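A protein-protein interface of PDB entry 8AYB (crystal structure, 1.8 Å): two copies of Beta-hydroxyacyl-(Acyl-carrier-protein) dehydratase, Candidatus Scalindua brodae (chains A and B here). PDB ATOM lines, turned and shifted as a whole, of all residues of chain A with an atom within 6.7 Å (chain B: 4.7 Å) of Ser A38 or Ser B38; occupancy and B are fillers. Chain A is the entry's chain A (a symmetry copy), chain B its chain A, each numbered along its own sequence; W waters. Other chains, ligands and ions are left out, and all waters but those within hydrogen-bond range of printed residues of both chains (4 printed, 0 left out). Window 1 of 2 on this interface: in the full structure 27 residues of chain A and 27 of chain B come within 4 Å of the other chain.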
ATOM      1  N   PHE A   3      -1.783  30.343  -1.986  1.00  0.00           N
ATOM      2  CA  PHE A   3      -1.322  31.341  -2.944  1.00  0.00           C
ATOM      3  C   PHE A   3      -0.958  32.649  -2.259  1.00  0.00           C
ATOM      4  O   PHE A   3       0.053  33.270  -2.602  1.00  0.00           O
ATOM      5  CB  PHE A   3      -2.386  31.582  -4.012  1.00  0.00           C
ATOM      6  CG  PHE A   3      -1.930  32.528  -5.097  1.00  0.00           C
ATOM      7  CD1 PHE A   3      -0.853  32.197  -5.902  1.00  0.00           C
ATOM      8  CD2 PHE A   3      -2.560  33.744  -5.294  1.00  0.00           C
ATOM      9  CE1 PHE A   3      -0.413  33.065  -6.898  1.00  0.00           C
ATOM     10  CE2 PHE A   3      -2.131  34.609  -6.287  1.00  0.00           C
ATOM     11  CZ  PHE A   3      -1.055  34.265  -7.093  1.00  0.00           C
ATOM     12  N   LEU A  17       4.451  35.133 -12.201  1.00  0.00           N
ATOM     13  CA  LEU A  17       4.468  34.276 -11.021  1.00  0.00           C
ATOM     14  C   LEU A  17       3.786  32.964 -11.389  1.00  0.00           C
ATOM     15  O   LEU A  17       2.609  32.960 -11.767  1.00  0.00           O
ATOM     16  CB  LEU A  17       3.774  34.951  -9.840  1.00  0.00           C
ATOM     17  CG  LEU A  17       3.518  34.042  -8.635  1.00  0.00           C
ATOM     18  CD1 LEU A  17       4.841  33.559  -8.065  1.00  0.00           C
ATOM     19  CD2 LEU A  17       2.719  34.807  -7.594  1.00  0.00           C
ATOM     20  N   ASP A  20       1.239  28.202  -7.703  1.00  0.00           N
ATOM     21  CA  ASP A  20      -0.035  28.421  -7.029  1.00  0.00           C
ATOM     22  C   ASP A  20      -0.005  28.032  -5.557  1.00  0.00           C
ATOM     23  O   ASP A  20      -0.543  28.760  -4.718  1.00  0.00           O
ATOM     24  CB  ASP A  20      -1.146  27.664  -7.749  1.00  0.00           C
ATOM     25  CG  ASP A  20      -1.545  28.350  -9.038  1.00  0.00           C
ATOM     26  OD1 ASP A  20      -1.776  29.584  -9.002  1.00  0.00           O
ATOM     27  OD2 ASP A  20      -1.600  27.672 -10.085  1.00  0.00           O
ATOM     28  N   LYS A  35       1.457  24.151  -9.854  1.00  0.00           N
ATOM     29  CA  LYS A  35       1.034  25.261 -10.703  1.00  0.00           C
ATOM     30  C   LYS A  35      -0.092  24.750 -11.584  1.00  0.00           C
ATOM     31  O   LYS A  35       0.121  23.852 -12.404  1.00  0.00           O
ATOM     32  CB  LYS A  35       2.183  25.807 -11.552  1.00  0.00           C
ATOM     33  CG  LYS A  35       1.695  27.032 -12.356  1.00  0.00           C
ATOM     34  CD  LYS A  35       2.425  27.187 -13.674  1.00  0.00           C
ATOM     35  CE  LYS A  35       1.944  28.435 -14.417  1.00  0.00           C
ATOM     36  NZ  LYS A  35       0.472  28.654 -14.290  1.00  0.00           N
ATOM     37  N   ASN A  36      -1.298  25.283 -11.392  1.00  0.00           N
ATOM     38  CA  ASN A  36      -2.386  24.993 -12.315  1.00  0.00           C
ATOM     39  C   ASN A  36      -2.099  25.622 -13.670  1.00  0.00           C
ATOM     40  O   ASN A  36      -1.704  26.794 -13.752  1.00  0.00           O
ATOM     41  CB  ASN A  36      -3.714  25.525 -11.773  1.00  0.00           C
ATOM     42  CG  ASN A  36      -4.392  24.547 -10.828  1.00  0.00           C
ATOM     43  OD1 ASN A  36      -3.964  23.397 -10.691  1.00  0.00           O
ATOM     44  ND2 ASN A  36      -5.453  24.997 -10.181  1.00  0.00           N
ATOM     45  N   ILE A  37      -2.310  24.858 -14.739  1.00  0.00           N
ATOM     46  CA  ILE A  37      -2.174  25.389 -16.092  1.00  0.00           C
ATOM     47  C   ILE A  37      -3.572  25.724 -16.594  1.00  0.00           C
ATOM     48  O   ILE A  37      -4.421  24.836 -16.738  1.00  0.00           O
ATOM     49  CB  ILE A  37      -1.462  24.404 -17.033  1.00  0.00           C
ATOM     50  CG1 ILE A  37      -0.180  23.850 -16.393  1.00  0.00           C
ATOM     51  CG2 ILE A  37      -1.151  25.094 -18.354  1.00  0.00           C
ATOM     52  CD1 ILE A  37       0.787  24.928 -15.906  1.00  0.00           C
ATOM     53  N   SER A  38      -3.819  27.006 -16.846  1.00  0.00           N
ATOM     54  CA  SER A  38      -5.123  27.498 -17.258  1.00  0.00           C
ATOM     55  C   SER A  38      -5.042  28.084 -18.654  1.00  0.00           C
ATOM     56  O   SER A  38      -4.136  28.870 -18.959  1.00  0.00           O
ATOM     57  CB  SER A  38      -5.633  28.549 -16.277  1.00  0.00           C
ATOM     58  OG  SER A  38      -6.712  29.268 -16.826  1.00  0.00           O
ATOM     59  N   GLY A  39      -6.006  27.724 -19.498  1.00  0.00           N
ATOM     60  CA  GLY A  39      -6.129  28.368 -20.797  1.00  0.00           C
ATOM     61  C   GLY A  39      -6.352  29.876 -20.739  1.00  0.00           C
ATOM     62  O   GLY A  39      -6.249  30.535 -21.778  1.00  0.00           O
ATOM     63  N   ASN A  40      -6.641  30.435 -19.563  1.00  0.00           N
ATOM     64  CA  ASN A  40      -6.868  31.869 -19.402  1.00  0.00           C
ATOM     65  C   ASN A  40      -5.597  32.598 -18.956  1.00  0.00           C
ATOM     66  O   ASN A  40      -5.673  33.733 -18.479  1.00  0.00           O
ATOM     67  CB  ASN A  40      -8.011  32.094 -18.402  1.00  0.00           C
ATOM     68  CG  ASN A  40      -8.506  33.535 -18.364  1.00  0.00           C
ATOM     69  OD1 ASN A  40      -8.688  34.182 -19.404  1.00  0.00           O
ATOM     70  ND2 ASN A  40      -8.747  34.041 -17.152  1.00  0.00           N
ATOM     71  N   GLU A  41      -4.425  31.957 -19.093  1.00  0.00           N
ATOM     72  CA  GLU A  41      -3.167  32.649 -18.780  1.00  0.00           C
ATOM     73  C   GLU A  41      -2.660  33.406 -20.004  1.00  0.00           C
ATOM     74  O   GLU A  41      -2.782  32.915 -21.128  1.00  0.00           O
ATOM     75  CB  GLU A  41      -2.102  31.669 -18.307  1.00  0.00           C
ATOM     76  CG  GLU A  41      -2.480  30.953 -16.991  1.00  0.00           C
ATOM     77  CD  GLU A  41      -1.420  29.997 -16.515  1.00  0.00           C
ATOM     78  OE1 GLU A  41      -0.306  30.460 -16.179  1.00  0.00           O
ATOM     79  OE2 GLU A  41      -1.709  28.771 -16.449  1.00  0.00           O
ATOM     80  N   PRO A  42      -2.103  34.607 -19.805  1.00  0.00           N
ATOM     81  CA  PRO A  42      -1.838  35.487 -20.955  1.00  0.00           C
ATOM     82  C   PRO A  42      -0.843  34.929 -21.952  1.00  0.00           C
ATOM     83  O   PRO A  42      -0.967  35.220 -23.146  1.00  0.00           O
ATOM     84  CB  PRO A  42      -1.332  36.789 -20.305  1.00  0.00           C
ATOM     85  CG  PRO A  42      -0.930  36.440 -18.934  1.00  0.00           C
ATOM     86  CD  PRO A  42      -1.827  35.266 -18.518  1.00  0.00           C
ATOM     87  N   PHE A  43       0.136  34.124 -21.515  1.00  0.00           N
ATOM     88  CA  PHE A  43       1.154  33.691 -22.466  1.00  0.00           C
ATOM     89  C   PHE A  43       0.600  32.735 -23.516  1.00  0.00           C
ATOM     90  O   PHE A  43       1.177  32.625 -24.599  1.00  0.00           O
ATOM     91  CB  PHE A  43       2.352  33.063 -21.736  1.00  0.00           C
ATOM     92  CG  PHE A  43       2.010  31.849 -20.908  1.00  0.00           C
ATOM     93  CD1 PHE A  43       1.832  30.615 -21.507  1.00  0.00           C
ATOM     94  CD2 PHE A  43       1.910  31.940 -19.533  1.00  0.00           C
ATOM     95  CE1 PHE A  43       1.511  29.485 -20.748  1.00  0.00           C
ATOM     96  CE2 PHE A  43       1.609  30.811 -18.762  1.00  0.00           C
ATOM     97  CZ  PHE A  43       1.412  29.583 -19.379  1.00  0.00           C
ATOM     98  N   PHE A  44      -0.508  32.043 -23.236  1.00  0.00           N
ATOM     99  CA  PHE A  44      -1.017  31.080 -24.208  1.00  0.00           C
ATOM    100  C   PHE A  44      -1.462  31.734 -25.513  1.00  0.00           C
ATOM    101  O   PHE A  44      -1.389  31.096 -26.573  1.00  0.00           O
ATOM    102  CB  PHE A  44      -2.168  30.284 -23.597  1.00  0.00           C
ATOM    103  CG  PHE A  44      -1.699  29.105 -22.786  1.00  0.00           C
ATOM    104  CD1 PHE A  44      -0.806  28.197 -23.335  1.00  0.00           C
ATOM    105  CD2 PHE A  44      -2.111  28.930 -21.473  1.00  0.00           C
ATOM    106  CE1 PHE A  44      -0.366  27.097 -22.601  1.00  0.00           C
ATOM    107  CE2 PHE A  44      -1.658  27.824 -20.726  1.00  0.00           C
ATOM    108  CZ  PHE A  44      -0.785  26.922 -21.300  1.00  0.00           C
ATOM    109  N   PHE A  99      -0.349  21.256 -21.174  1.00  0.00           N
ATOM    110  CA  PHE A  99      -1.494  21.886 -21.819  1.00  0.00           C
ATOM    111  C   PHE A  99      -2.415  22.532 -20.798  1.00  0.00           C
ATOM    112  O   PHE A  99      -2.425  22.139 -19.628  1.00  0.00           O
ATOM    113  CB  PHE A  99      -2.300  20.857 -22.630  1.00  0.00           C
ATOM    114  CG  PHE A  99      -1.515  20.225 -23.730  1.00  0.00           C
ATOM    115  CD1 PHE A  99      -1.207  20.945 -24.875  1.00  0.00           C
ATOM    116  CD2 PHE A  99      -1.047  18.929 -23.606  1.00  0.00           C
ATOM    117  CE1 PHE A  99      -0.452  20.373 -25.887  1.00  0.00           C
ATOM    118  CE2 PHE A  99      -0.298  18.353 -24.610  1.00  0.00           C
ATOM    119  CZ  PHE A  99      -0.001  19.071 -25.752  1.00  0.00           C
ATOM    120  N   PRO A 100      -3.225  23.507 -21.217  1.00  0.00           N
ATOM    121  CA  PRO A 100      -4.325  23.960 -20.358  1.00  0.00           C
ATOM    122  C   PRO A 100      -5.129  22.772 -19.839  1.00  0.00           C
ATOM    123  O   PRO A 100      -5.434  21.834 -20.576  1.00  0.00           O
ATOM    124  CB  PRO A 100      -5.146  24.851 -21.293  1.00  0.00           C
ATOM    125  CG  PRO A 100      -4.079  25.439 -22.226  1.00  0.00           C
ATOM    126  CD  PRO A 100      -3.181  24.258 -22.489  1.00  0.00           C
ATOM    127  N   GLY A 101      -5.442  22.806 -18.547  1.00  0.00           N
ATOM    128  CA  GLY A 101      -6.093  21.703 -17.874  1.00  0.00           C
ATOM    129  C   GLY A 101      -5.153  20.840 -17.065  1.00  0.00           C
ATOM    130  O   GLY A 101      -5.614  20.118 -16.169  1.00  0.00           O
ATOM    131  N   ASP A 102      -3.853  20.901 -17.352  1.00  0.00           N
ATOM    132  CA  ASP A 102      -2.864  20.125 -16.609  1.00  0.00           C
ATOM    133  C   ASP A 102      -2.599  20.745 -15.245  1.00  0.00           C
ATOM    134  O   ASP A 102      -2.586  21.970 -15.092  1.00  0.00           O
ATOM    135  CB  ASP A 102      -1.544  20.037 -17.374  1.00  0.00           C
ATOM    136  CG  ASP A 102      -1.601  19.081 -18.541  1.00  0.00           C
ATOM    137  OD1 ASP A 102      -2.570  18.285 -18.627  1.00  0.00           O
ATOM    138  OD2 ASP A 102      -0.656  19.108 -19.355  1.00  0.00           O
ATOM    139  N   ASP B  20     -11.330  24.652 -19.345  1.00  0.00           N
ATOM    140  CA  ASP B  20     -10.105  24.043 -19.848  1.00  0.00           C
ATOM    141  C   ASP B  20     -10.348  22.724 -20.570  1.00  0.00           C
ATOM    142  O   ASP B  20      -9.748  22.480 -21.622  1.00  0.00           O
ATOM    143  CB  ASP B  20      -9.113  23.842 -18.707  1.00  0.00           C
ATOM    144  CG  ASP B  20      -8.467  25.146 -18.292  1.00  0.00           C
ATOM    145  OD1 ASP B  20      -7.990  25.880 -19.193  1.00  0.00           O
ATOM    146  OD2 ASP B  20      -8.458  25.452 -17.081  1.00  0.00           O
ATOM    147  N   LYS B  35     -12.182  23.607 -14.955  1.00  0.00           N
ATOM    148  CA  LYS B  35     -11.465  24.863 -15.146  1.00  0.00           C
ATOM    149  C   LYS B  35     -10.394  24.937 -14.073  1.00  0.00           C
ATOM    150  O   LYS B  35     -10.711  24.989 -12.881  1.00  0.00           O
ATOM    151  CB  LYS B  35     -12.395  26.075 -15.070  1.00  0.00           C
ATOM    152  CG  LYS B  35     -11.595  27.361 -15.368  1.00  0.00           C
ATOM    153  CD  LYS B  35     -12.155  28.571 -14.650  1.00  0.00           C
ATOM    154  CE  LYS B  35     -11.363  29.830 -15.008  1.00  0.00           C
ATOM    155  NZ  LYS B  35      -9.894  29.579 -15.121  1.00  0.00           N
ATOM    156  N   ASN B  36      -9.126  24.900 -14.482  1.00  0.00           N
ATOM    157  CA  ASN B  36      -8.043  25.156 -13.544  1.00  0.00           C
ATOM    158  C   ASN B  36      -8.070  26.613 -13.106  1.00  0.00           C
ATOM    159  O   ASN B  36      -8.206  27.521 -13.937  1.00  0.00           O
ATOM    160  CB  ASN B  36      -6.688  24.838 -14.180  1.00  0.00           C
ATOM    161  CG  ASN B  36      -6.313  23.371 -14.051  1.00  0.00           C
ATOM    162  OD1 ASN B  36      -6.979  22.606 -13.347  1.00  0.00           O
ATOM    163  ND2 ASN B  36      -5.245  22.975 -14.723  1.00  0.00           N
ATOM    164  N   ILE B  37      -7.924  26.846 -11.804  1.00  0.00           N
ATOM    165  CA  ILE B  37      -7.825  28.205 -11.281  1.00  0.00           C
ATOM    166  C   ILE B  37      -6.349  28.501 -11.057  1.00  0.00           C
ATOM    167  O   ILE B  37      -5.692  27.850 -10.236  1.00  0.00           O
ATOM    168  CB  ILE B  37      -8.636  28.390  -9.988  1.00  0.00           C
ATOM    169  CG1 ILE B  37     -10.057  27.826 -10.138  1.00  0.00           C
ATOM    170  CG2 ILE B  37      -8.678  29.867  -9.620  1.00  0.00           C
ATOM    171  CD1 ILE B  37     -10.822  28.377 -11.340  1.00  0.00           C
ATOM    172  N   SER B  38      -5.822  29.474 -11.794  1.00  0.00           N
ATOM    173  CA  SER B  38      -4.413  29.827 -11.754  1.00  0.00           C
ATOM    174  C   SER B  38      -4.245  31.243 -11.237  1.00  0.00           C
ATOM    175  O   SER B  38      -4.938  32.166 -11.683  1.00  0.00           O
ATOM    176  CB  SER B  38      -3.788  29.697 -13.139  1.00  0.00           C
ATOM    177  OG  SER B  38      -2.539  30.346 -13.191  1.00  0.00           O
ATOM    178  N   GLY B  39      -3.303  31.421 -10.314  1.00  0.00           N
ATOM    179  CA  GLY B  39      -2.932  32.763  -9.887  1.00  0.00           C
ATOM    180  C   GLY B  39      -2.410  33.663 -11.002  1.00  0.00           C
ATOM    181  O   GLY B  39      -2.282  34.870 -10.783  1.00  0.00           O
ATOM    182  N   ASN B  40      -2.120  33.115 -12.183  1.00  0.00           N
ATOM    183  CA  ASN B  40      -1.618  33.890 -13.315  1.00  0.00           C
ATOM    184  C   ASN B  40      -2.747  34.305 -14.263  1.00  0.00           C
ATOM    185  O   ASN B  40      -2.483  34.686 -15.406  1.00  0.00           O
ATOM    186  CB  ASN B  40      -0.549  33.075 -14.055  1.00  0.00           C
ATOM    187  CG  ASN B  40       0.227  33.890 -15.084  1.00  0.00           C
ATOM    188  OD1 ASN B  40       0.631  35.032 -14.830  1.00  0.00           O
ATOM    189  ND2 ASN B  40       0.457  33.290 -16.256  1.00  0.00           N
ATOM    190  N   GLU B  41      -4.008  34.226 -13.810  1.00  0.00           N
ATOM    191  CA  GLU B  41      -5.121  34.711 -14.640  1.00  0.00           C
ATOM    192  C   GLU B  41      -5.348  36.201 -14.403  1.00  0.00           C
ATOM    193  O   GLU B  41      -5.228  36.670 -13.269  1.00  0.00           O
ATOM    194  CB  GLU B  41      -6.403  33.944 -14.345  1.00  0.00           C
ATOM    195  CG  GLU B  41      -6.300  32.441 -14.687  1.00  0.00           C
ATOM    196  CD  GLU B  41      -7.573  31.686 -14.412  1.00  0.00           C
ATOM    197  OE1 GLU B  41      -8.594  31.975 -15.077  1.00  0.00           O
ATOM    198  OE2 GLU B  41      -7.550  30.775 -13.539  1.00  0.00           O
ATOM    199  N   PHE B  44      -7.433  38.100 -11.407  1.00  0.00           N
ATOM    200  CA  PHE B  44      -7.048  38.072  -9.999  1.00  0.00           C
ATOM    201  C   PHE B  44      -6.362  39.357  -9.545  1.00  0.00           C
ATOM    202  O   PHE B  44      -6.467  39.725  -8.367  1.00  0.00           O
ATOM    203  CB  PHE B  44      -6.145  36.869  -9.732  1.00  0.00           C
ATOM    204  CG  PHE B  44      -6.918  35.603  -9.469  1.00  0.00           C
ATOM    205  CD1 PHE B  44      -7.925  35.591  -8.516  1.00  0.00           C
ATOM    206  CD2 PHE B  44      -6.671  34.450 -10.199  1.00  0.00           C
ATOM    207  CE1 PHE B  44      -8.647  34.428  -8.256  1.00  0.00           C
ATOM    208  CE2 PHE B  44      -7.408  33.275  -9.944  1.00  0.00           C
ATOM    209  CZ  PHE B  44      -8.392  33.281  -8.976  1.00  0.00           C
ATOM    210  N   PRO B 100      -6.725  30.481  -6.329  1.00  0.00           N
ATOM    211  CA  PRO B 100      -5.638  29.928  -7.144  1.00  0.00           C
ATOM    212  C   PRO B 100      -5.145  28.607  -6.561  1.00  0.00           C
ATOM    213  O   PRO B 100      -4.975  28.464  -5.349  1.00  0.00           O
ATOM    214  CB  PRO B 100      -4.570  31.022  -7.081  1.00  0.00           C
ATOM    215  CG  PRO B 100      -5.404  32.306  -6.970  1.00  0.00           C
ATOM    216  CD  PRO B 100      -6.498  31.908  -6.014  1.00  0.00           C
HETATM  217  O   HOH W   1      -4.292  29.055  -2.673  1.00  0.00           O
HETATM  218  O   HOH W   2       1.501  35.313 -12.551  1.00  0.00           O
HETATM  219  O   HOH W   3      -0.589  29.487 -11.927  1.00  0.00           O
HETATM  220  O   HOH W   4      -8.903  28.188 -17.239  1.00  0.00           O
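Lys A35 touches Ser B38, and with the chains exchanged Ser A38 touches Lys B35.
Asn A36 touches Ile B37, and with the chains exchanged Ile A37 touches Asn B36.
Ser A38 touches Glu B41, and with the chains exchanged Glu A41 touches Ser B38.
Asn A40 touches Glu B41, and with the chains exchanged Glu A41 touches Asn B40.
Positions printed for both chains: 20, 35, 36, 37, 38, 39, 40, 41, 44 and 100.
The backbone carbonyl oxygen (O) of Ile A37 sits at hydrogen-bond distance from the side-chain amide nitrogen (ND2) of Asn B36.
The backbone NH (N) of Gly B39 sits at hydrogen-bond distance from the side-chain carboxylate (OD1) of Asp A20 (2.7 Å).
OD1 of Asp B20 sits at hydrogen-bond distance from N of Gly A39, at 2.7 Å.
O of Asp A102 sits at hydrogen-bond distance from ND2 of Asn B36, at 2.9 Å.
The backbone carbonyl oxygen (O) of Ile B37 sits at hydrogen-bond distance from the side-chain amide nitrogen (ND2) of Asn A36 (2.9 Å).
The backbone carbonyl oxygen (O) of Gly A101 sits close to the side-chain amide nitrogen (ND2) of Asn B36 (3.2 Å).
ND2 of Asn B40 lies within hydrogen-bond range of OE1 of Glu A41, 2.9 Å away.
ND2 of Asn A40 lies within hydrogen-bond range of OE1 of Glu B41 (2.9 Å).
Among the printed residues, 26 pairs touch across the chains.
CZ of Phe A3 touches CA of Gly B39 (3.7 Å).
C of Ser B38 touches OD1 of Asp A20, at 3.7 Å.
Pro B100 touches Asp A20 (CB to OD1, 3.7 Å).
Ser B38 touches Asn A36 (CB to O, 3.6 Å).
Asp B20 touches Ser A38 (OD1 to C, 3.7 Å).
Ser A38 touches Lys B35 (OG to NZ, 3.6 Å).
CB of Ser A38 touches O of Asn B36, at 3.6 Å.
CB of Ser B38 touches CB of Ser A38, 3.8 Å away.
Ser B38 touches Glu A41.
Pro A100 touches Asp B20.
Water W2 bridges the side-chain amide oxygen (OD1) of Asn B40 (2.5 Å) and the backbone carbonyl oxygen (O) of Leu A17 (2.7 Å).
Water W4 lies within hydrogen-bond range of OG of Ser A38 (2.5 Å), NZ of Lys B35 (2.7 Å), OD2 of Asp B20 (2.8 Å) and O of Asn B36 (3.4 Å).
Water W3 lies within hydrogen-bond range of the side-chain hydroxyl (OG) of Ser B38 (2.5 Å), the side-chain amino group (NZ) of Lys A35 (2.7 Å), the side-chain carboxylate (OD2) of Asp A20 (2.8 Å) and the backbone carbonyl oxygen (O) of Asn A36 (3.4 Å).
Water W1 bridges O of Pro B100 (2.8 Å) and N of Phe A3 (2.9 Å).
Of the printed residues of chain B, Asp A20 touches Ser B38, Gly B39 and Pro B100.
Of the printed residues of chain B, Lys A35 touches Ser B38.
Of the printed residues of chain B, Ser A38 touches Asp B20 (3.7 Å), Lys B35 (3.6 Å), Asn B36 (3.6 Å), Ser B38 (3.8 Å) and Glu B41 (3.5 Å).
Phe A99 touches none of the printed residues of chain B.
Printed residues of chain A within 4 Å of Ser B38: Asp A20 (3.7 Å), Lys A35 (3.6 Å), Asn A36 (3.6 Å), Ser A38 (3.8 Å) and Glu A41 (3.5 Å).
Of the printed residues of chain A, Asn B40 touches Leu A17, Glu A41, Pro A42 and Phe A43.
The nearest printed residue of chain B that does not touch Ile A37 is Asp B20 (4.1 Å).
The backbone NH of Asn A36 sits at hydrogen-bond distance from the side-chain carboxylate of Asp A20 (2.7 Å).
The backbone NH (N) of Ser B38 sits at hydrogen-bond distance from the side-chain carboxylate (OE2) of Glu B41, 2.8 Å away.
The side-chain amino group of Lys B35 lies within salt-bridge range of the side-chain carboxylate of Glu B41, 2.7 Å away.
The backbone carbonyl oxygen (O) of Asp A20 lies close to the backbone NH (N) of Phe A3, at 3.4 Å.
The backbone NH of Phe A99 is in hydrogen-bond range of the side-chain carboxylate of Asp A102, at 2.8 Å.
The side-chain hydroxyl (OG) of Ser A38 is in hydrogen-bond range of the backbone NH (N) of Asn A40 (3.0 Å).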
